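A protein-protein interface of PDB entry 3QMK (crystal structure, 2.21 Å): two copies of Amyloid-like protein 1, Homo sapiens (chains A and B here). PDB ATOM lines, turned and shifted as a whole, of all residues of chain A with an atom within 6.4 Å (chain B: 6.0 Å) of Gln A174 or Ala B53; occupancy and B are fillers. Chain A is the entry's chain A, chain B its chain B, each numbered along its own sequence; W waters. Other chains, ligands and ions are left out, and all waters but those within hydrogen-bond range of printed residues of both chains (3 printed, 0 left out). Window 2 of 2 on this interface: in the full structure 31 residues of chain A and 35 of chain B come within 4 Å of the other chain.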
ATOM      1  N   VAL A 169     -28.049  -3.133  19.554  1.00  0.00           N
ATOM      2  CA  VAL A 169     -27.189  -4.030  18.793  1.00  0.00           C
ATOM      3  C   VAL A 169     -27.703  -4.108  17.351  1.00  0.00           C
ATOM      4  O   VAL A 169     -26.921  -3.971  16.404  1.00  0.00           O
ATOM      5  CB  VAL A 169     -27.163  -5.469  19.418  1.00  0.00           C
ATOM      6  CG1 VAL A 169     -26.409  -6.426  18.504  1.00  0.00           C
ATOM      7  CG2 VAL A 169     -26.512  -5.434  20.808  1.00  0.00           C
ATOM      8  N   HIS A 170     -29.016  -4.310  17.197  1.00  0.00           N
ATOM      9  CA  HIS A 170     -29.670  -4.407  15.878  1.00  0.00           C
ATOM     10  C   HIS A 170     -29.273  -3.199  14.997  1.00  0.00           C
ATOM     11  O   HIS A 170     -28.813  -3.349  13.867  1.00  0.00           O
ATOM     12  CB  HIS A 170     -31.198  -4.456  16.093  1.00  0.00           C
ATOM     13  CG  HIS A 170     -32.014  -4.571  14.839  1.00  0.00           C
ATOM     14  ND1 HIS A 170     -31.662  -5.391  13.783  1.00  0.00           N
ATOM     15  CD2 HIS A 170     -33.206  -4.016  14.503  1.00  0.00           C
ATOM     16  CE1 HIS A 170     -32.604  -5.336  12.854  1.00  0.00           C
ATOM     17  NE2 HIS A 170     -33.551  -4.508  13.269  1.00  0.00           N
ATOM     18  N   THR A 171     -29.448  -2.011  15.558  1.00  0.00           N
ATOM     19  CA  THR A 171     -29.139  -0.756  14.893  1.00  0.00           C
ATOM     20  C   THR A 171     -27.652  -0.588  14.569  1.00  0.00           C
ATOM     21  O   THR A 171     -27.304  -0.238  13.447  1.00  0.00           O
ATOM     22  CB  THR A 171     -29.593   0.413  15.770  1.00  0.00           C
ATOM     23  OG1 THR A 171     -31.001   0.296  16.015  1.00  0.00           O
ATOM     24  CG2 THR A 171     -29.303   1.741  15.093  1.00  0.00           C
ATOM     25  N   HIS A 172     -26.778  -0.851  15.539  1.00  0.00           N
ATOM     26  CA  HIS A 172     -25.339  -0.700  15.332  1.00  0.00           C
ATOM     27  C   HIS A 172     -24.781  -1.638  14.260  1.00  0.00           C
ATOM     28  O   HIS A 172     -23.939  -1.242  13.455  1.00  0.00           O
ATOM     29  CB  HIS A 172     -24.590  -0.893  16.655  1.00  0.00           C
ATOM     30  CG  HIS A 172     -23.125  -0.579  16.576  1.00  0.00           C
ATOM     31  ND1 HIS A 172     -22.284  -0.688  17.664  1.00  0.00           N
ATOM     32  CD2 HIS A 172     -22.347  -0.179  15.542  1.00  0.00           C
ATOM     33  CE1 HIS A 172     -21.052  -0.372  17.300  1.00  0.00           C
ATOM     34  NE2 HIS A 172     -21.064  -0.060  16.018  1.00  0.00           N
ATOM     35  N   LEU A 173     -25.245  -2.882  14.242  1.00  0.00           N
ATOM     36  CA  LEU A 173     -24.775  -3.818  13.237  1.00  0.00           C
ATOM     37  C   LEU A 173     -25.156  -3.322  11.836  1.00  0.00           C
ATOM     38  O   LEU A 173     -24.397  -3.506  10.879  1.00  0.00           O
ATOM     39  CB  LEU A 173     -25.355  -5.216  13.498  1.00  0.00           C
ATOM     40  CG  LEU A 173     -24.810  -5.902  14.758  1.00  0.00           C
ATOM     41  CD1 LEU A 173     -25.609  -7.168  15.050  1.00  0.00           C
ATOM     42  CD2 LEU A 173     -23.331  -6.232  14.564  1.00  0.00           C
ATOM     43  N   GLN A 174     -26.327  -2.700  11.711  1.00  0.00           N
ATOM     44  CA  GLN A 174     -26.743  -2.186  10.404  1.00  0.00           C
ATOM     45  C   GLN A 174     -25.858  -0.995  10.008  1.00  0.00           C
ATOM     46  O   GLN A 174     -25.464  -0.862   8.848  1.00  0.00           O
ATOM     47  CB  GLN A 174     -28.219  -1.771  10.423  1.00  0.00           C
ATOM     48  CG  GLN A 174     -29.199  -2.925  10.301  1.00  0.00           C
ATOM     49  CD  GLN A 174     -30.639  -2.493  10.554  1.00  0.00           C
ATOM     50  OE1 GLN A 174     -31.015  -2.170  11.685  1.00  0.00           O
ATOM     51  NE2 GLN A 174     -31.451  -2.482   9.499  1.00  0.00           N
ATOM     52  N   VAL A 175     -25.535  -0.150  10.981  1.00  0.00           N
ATOM     53  CA  VAL A 175     -24.678   1.004  10.734  1.00  0.00           C
ATOM     54  C   VAL A 175     -23.368   0.520  10.118  1.00  0.00           C
ATOM     55  O   VAL A 175     -22.944   1.015   9.072  1.00  0.00           O
ATOM     56  CB  VAL A 175     -24.387   1.764  12.052  1.00  0.00           C
ATOM     57  CG1 VAL A 175     -23.257   2.772  11.854  1.00  0.00           C
ATOM     58  CG2 VAL A 175     -25.656   2.479  12.517  1.00  0.00           C
ATOM     59  N   ILE A 176     -22.746  -0.473  10.749  1.00  0.00           N
ATOM     60  CA  ILE A 176     -21.482  -1.011  10.251  1.00  0.00           C
ATOM     61  C   ILE A 176     -21.608  -1.526   8.823  1.00  0.00           C
ATOM     62  O   ILE A 176     -20.745  -1.287   7.973  1.00  0.00           O
ATOM     63  CB  ILE A 176     -20.970  -2.183  11.127  1.00  0.00           C
ATOM     64  CG1 ILE A 176     -20.698  -1.705  12.554  1.00  0.00           C
ATOM     65  CG2 ILE A 176     -19.717  -2.764  10.516  1.00  0.00           C
ATOM     66  CD1 ILE A 176     -20.407  -2.849  13.551  1.00  0.00           C
ATOM     67  N   GLU A 177     -22.689  -2.244   8.560  1.00  0.00           N
ATOM     68  CA  GLU A 177     -22.882  -2.808   7.237  1.00  0.00           C
ATOM     69  C   GLU A 177     -23.089  -1.731   6.175  1.00  0.00           C
ATOM     70  O   GLU A 177     -22.630  -1.877   5.044  1.00  0.00           O
ATOM     71  CB  GLU A 177     -24.051  -3.777   7.259  1.00  0.00           C
ATOM     72  CG  GLU A 177     -23.869  -4.906   6.292  1.00  0.00           C
ATOM     73  CD  GLU A 177     -25.043  -5.026   5.362  1.00  0.00           C
ATOM     74  OE1 GLU A 177     -25.340  -4.031   4.664  1.00  0.00           O
ATOM     75  OE2 GLU A 177     -25.670  -6.107   5.341  1.00  0.00           O
ATOM     76  N   GLU A 178     -23.766  -0.644   6.539  1.00  0.00           N
ATOM     77  CA  GLU A 178     -23.981   0.453   5.598  1.00  0.00           C
ATOM     78  C   GLU A 178     -22.667   1.183   5.329  1.00  0.00           C
ATOM     79  O   GLU A 178     -22.406   1.605   4.200  1.00  0.00           O
ATOM     80  CB  GLU A 178     -25.032   1.428   6.134  1.00  0.00           C
ATOM     81  N   ARG A 179     -21.857   1.346   6.376  1.00  0.00           N
ATOM     82  CA  ARG A 179     -20.562   2.004   6.248  1.00  0.00           C
ATOM     83  C   ARG A 179     -19.739   1.209   5.247  1.00  0.00           C
ATOM     84  O   ARG A 179     -19.164   1.762   4.315  1.00  0.00           O
ATOM     85  CB  ARG A 179     -19.829   2.024   7.589  1.00  0.00           C
ATOM     86  CG  ARG A 179     -19.680   3.392   8.232  1.00  0.00           C
ATOM     87  CD  ARG A 179     -18.368   3.457   9.023  1.00  0.00           C
ATOM     88  NE  ARG A 179     -18.185   2.299   9.894  1.00  0.00           N
ATOM     89  CZ  ARG A 179     -18.562   2.242  11.168  1.00  0.00           C
ATOM     90  NH1 ARG A 179     -19.151   3.291  11.725  1.00  0.00           N
ATOM     91  NH2 ARG A 179     -18.333   1.143  11.886  1.00  0.00           N
ATOM     92  N   VAL B  48     -29.621 -13.932  13.157  1.00  0.00           N
ATOM     93  CA  VAL B  48     -30.929 -13.440  13.549  1.00  0.00           C
ATOM     94  C   VAL B  48     -31.007 -11.947  13.247  1.00  0.00           C
ATOM     95  O   VAL B  48     -31.958 -11.484  12.606  1.00  0.00           O
ATOM     96  CB  VAL B  48     -31.206 -13.700  15.047  1.00  0.00           C
ATOM     97  CG1 VAL B  48     -32.569 -13.110  15.447  1.00  0.00           C
ATOM     98  CG2 VAL B  48     -31.234 -15.205  15.302  1.00  0.00           C
ATOM     99  N   MET B  49     -29.994 -11.208  13.692  1.00  0.00           N
ATOM    100  CA  MET B  49     -29.924  -9.762  13.482  1.00  0.00           C
ATOM    101  C   MET B  49     -30.025  -9.379  12.002  1.00  0.00           C
ATOM    102  O   MET B  49     -30.671  -8.393  11.668  1.00  0.00           O
ATOM    103  CB  MET B  49     -28.629  -9.178  14.077  1.00  0.00           C
ATOM    104  CG  MET B  49     -28.573  -9.169  15.599  1.00  0.00           C
ATOM    105  SD  MET B  49     -29.765  -8.061  16.401  1.00  0.00           S
ATOM    106  CE  MET B  49     -29.543  -8.529  18.139  1.00  0.00           C
ATOM    107  N   ARG B  50     -29.407 -10.153  11.118  1.00  0.00           N
ATOM    108  CA  ARG B  50     -29.488  -9.849   9.689  1.00  0.00           C
ATOM    109  C   ARG B  50     -30.904 -10.075   9.152  1.00  0.00           C
ATOM    110  O   ARG B  50     -31.390  -9.292   8.352  1.00  0.00           O
ATOM    111  CB  ARG B  50     -28.473 -10.684   8.900  1.00  0.00           C
ATOM    112  CG  ARG B  50     -27.036 -10.450   9.333  1.00  0.00           C
ATOM    113  CD  ARG B  50     -26.039 -10.838   8.257  1.00  0.00           C
ATOM    114  NE  ARG B  50     -26.045  -9.861   7.173  1.00  0.00           N
ATOM    115  CZ  ARG B  50     -25.148  -9.817   6.193  1.00  0.00           C
ATOM    116  NH1 ARG B  50     -24.157 -10.695   6.153  1.00  0.00           N
ATOM    117  NH2 ARG B  50     -25.237  -8.883   5.255  1.00  0.00           N
ATOM    118  N   GLU B  51     -31.561 -11.142   9.596  1.00  0.00           N
ATOM    119  CA  GLU B  51     -32.929 -11.440   9.171  1.00  0.00           C
ATOM    120  C   GLU B  51     -33.867 -10.315   9.602  1.00  0.00           C
ATOM    121  O   GLU B  51     -34.681  -9.816   8.825  1.00  0.00           O
ATOM    122  CB  GLU B  51     -33.426 -12.718   9.819  1.00  0.00           C
ATOM    123  CG  GLU B  51     -33.437 -13.913   8.918  1.00  0.00           C
ATOM    124  CD  GLU B  51     -34.408 -14.957   9.402  1.00  0.00           C
ATOM    125  OE1 GLU B  51     -35.599 -14.919   9.001  1.00  0.00           O
ATOM    126  OE2 GLU B  51     -33.971 -15.808  10.202  1.00  0.00           O
ATOM    127  N   TRP B  52     -33.758  -9.942  10.869  1.00  0.00           N
ATOM    128  CA  TRP B  52     -34.564  -8.882  11.443  1.00  0.00           C
ATOM    129  C   TRP B  52     -34.412  -7.586  10.634  1.00  0.00           C
ATOM    130  O   TRP B  52     -35.395  -6.891  10.378  1.00  0.00           O
ATOM    131  CB  TRP B  52     -34.127  -8.664  12.888  1.00  0.00           C
ATOM    132  CG  TRP B  52     -34.972  -7.746  13.678  1.00  0.00           C
ATOM    133  CD1 TRP B  52     -36.170  -7.204  13.317  1.00  0.00           C
ATOM    134  CD2 TRP B  52     -34.692  -7.266  14.997  1.00  0.00           C
ATOM    135  NE1 TRP B  52     -36.656  -6.411  14.333  1.00  0.00           N
ATOM    136  CE2 TRP B  52     -35.765  -6.433  15.375  1.00  0.00           C
ATOM    137  CE3 TRP B  52     -33.630  -7.464  15.894  1.00  0.00           C
ATOM    138  CZ2 TRP B  52     -35.813  -5.795  16.615  1.00  0.00           C
ATOM    139  CZ3 TRP B  52     -33.672  -6.832  17.122  1.00  0.00           C
ATOM    140  CH2 TRP B  52     -34.762  -6.003  17.473  1.00  0.00           C
ATOM    141  N   ALA B  53     -33.183  -7.266  10.237  1.00  0.00           N
ATOM    142  CA  ALA B  53     -32.931  -6.054   9.463  1.00  0.00           C
ATOM    143  C   ALA B  53     -33.644  -6.150   8.118  1.00  0.00           C
ATOM    144  O   ALA B  53     -34.310  -5.203   7.686  1.00  0.00           O
ATOM    145  CB  ALA B  53     -31.427  -5.856   9.245  1.00  0.00           C
ATOM    146  N   MET B  54     -33.503  -7.303   7.467  1.00  0.00           N
ATOM    147  CA  MET B  54     -34.138  -7.535   6.186  1.00  0.00           C
ATOM    148  C   MET B  54     -35.644  -7.378   6.357  1.00  0.00           C
ATOM    149  O   MET B  54     -36.292  -6.732   5.538  1.00  0.00           O
ATOM    150  CB  MET B  54     -33.801  -8.931   5.676  1.00  0.00           C
ATOM    151  N   ALA B  55     -36.201  -7.959   7.421  1.00  0.00           N
ATOM    152  CA  ALA B  55     -37.638  -7.834   7.659  1.00  0.00           C
ATOM    153  C   ALA B  55     -38.028  -6.360   7.792  1.00  0.00           C
ATOM    154  O   ALA B  55     -39.055  -5.940   7.251  1.00  0.00           O
ATOM    155  CB  ALA B  55     -38.048  -8.590   8.903  1.00  0.00           C
ATOM    156  N   ASP B  56     -37.214  -5.587   8.513  1.00  0.00           N
ATOM    157  CA  ASP B  56     -37.477  -4.158   8.679  1.00  0.00           C
ATOM    158  C   ASP B  56     -37.587  -3.498   7.313  1.00  0.00           C
ATOM    159  O   ASP B  56     -38.444  -2.645   7.099  1.00  0.00           O
ATOM    160  CB  ASP B  56     -36.353  -3.452   9.447  1.00  0.00           C
ATOM    161  CG  ASP B  56     -36.380  -3.732  10.928  1.00  0.00           C
ATOM    162  OD1 ASP B  56     -37.445  -4.088  11.474  1.00  0.00           O
ATOM    163  OD2 ASP B  56     -35.318  -3.576  11.557  1.00  0.00           O
ATOM    164  N   ASN B  57     -36.699  -3.886   6.402  1.00  0.00           N
ATOM    165  CA  ASN B  57     -36.708  -3.339   5.051  1.00  0.00           C
ATOM    166  C   ASN B  57     -38.014  -3.691   4.362  1.00  0.00           C
ATOM    167  O   ASN B  57     -38.785  -2.806   3.993  1.00  0.00           O
ATOM    168  CB  ASN B  57     -35.540  -3.900   4.236  1.00  0.00           C
ATOM    169  CG  ASN B  57     -34.222  -3.252   4.587  1.00  0.00           C
ATOM    170  OD1 ASN B  57     -34.043  -2.049   4.397  1.00  0.00           O
ATOM    171  ND2 ASN B  57     -33.287  -4.043   5.108  1.00  0.00           N
ATOM    172  N   GLN B  58     -38.254  -4.988   4.210  1.00  0.00           N
ATOM    173  CA  GLN B  58     -39.455  -5.516   3.564  1.00  0.00           C
ATOM    174  C   GLN B  58     -40.800  -5.063   4.118  1.00  0.00           C
ATOM    175  O   GLN B  58     -41.768  -4.962   3.374  1.00  0.00           O
ATOM    176  CB  GLN B  58     -39.469  -7.049   3.627  1.00  0.00           C
ATOM    177  CG  GLN B  58     -38.732  -7.786   2.542  1.00  0.00           C
ATOM    178  CD  GLN B  58     -39.226  -9.225   2.413  1.00  0.00           C
ATOM    179  OE1 GLN B  58     -39.278  -9.976   3.392  1.00  0.00           O
ATOM    180  NE2 GLN B  58     -39.596  -9.612   1.199  1.00  0.00           N
HETATM  181  O   HOH W   1     -31.729  -2.546   6.880  1.00  0.00           O
HETATM  182  O   HOH W   2     -33.721  -1.562  10.696  1.00  0.00           O
HETATM  183  O   HOH W   3     -29.165  -5.890  12.702  1.00  0.00           O
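The side-chain amide oxygen of Gln A174 sits close to the backbone carbonyl oxygen of His A170 (3.3 Å). O of Ala B53 sits at hydrogen-bond distance from ND2 of Asn B57.
Of the printed residues of chain B, His A170 touches Met B49, Trp B52, Ala B53 and Asp B56. Thr A171 touches none of the printed residues of chain B. Gln A174 touches just one residue of chain B: Ala B53 (3.4 Å). Of the printed residues of chain A, Trp B52 touches His A170 (3.4 Å). Ala B53 touches just these residues of chain A: His A170 and Gln A174. Met B54 touches none of the printed residues of chain A. Printed residues of chain A within 4 Å of Asp B56: His A170 (2.6 Å). The nearest residue of chain B that does not touch Gln A174 is Asp B56 (4.5 Å).
The side-chain carboxylate of Asp B56 lies within hydrogen-bond range of a ring nitrogen (NE2) of His A170 (2.6 Å). The side-chain carboxylate (OE2) of Glu A177 lies within salt-bridge range of the guanidinium group (NH2) of Arg B50, 2.8 Å away.
Water W1 bridges NE2 of Gln A174 and ND2 of Asn B57. Water W2 bridges the side-chain carboxylate (OD2) of Asp B56 (2.7 Å) and the side-chain amide nitrogen (NE2) of Gln A174 (2.7 Å). Water W3 bridges ND1 of His A170 and O of Met B49.
Of the 11 printed residues of chain B, 5 touch a printed residue of chain A. Of the 11 printed residues of chain A, 5 touch a printed residue of chain B. Hydrophobic or aromatic side chains of chain A that line the printed part of chain B: Val A169, His A170 and Leu A173. Among the printed residues, 8 pairs touch across the chains. Among the printed residues, Asp or Glu carboxylates within 4 Å of a Lys or Arg side-chain nitrogen of the other chain: Glu A177 with Arg B50 (2.8 Å).
Among the printed residues, merely in contact across the chains: His A170 with Ala B53, Gln A174 with Ala B53, His A170 with Trp B52, Leu A173 with Met B49, His A170 with Met B49 and Val A169 with Met B49.
No position is printed for both chains.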
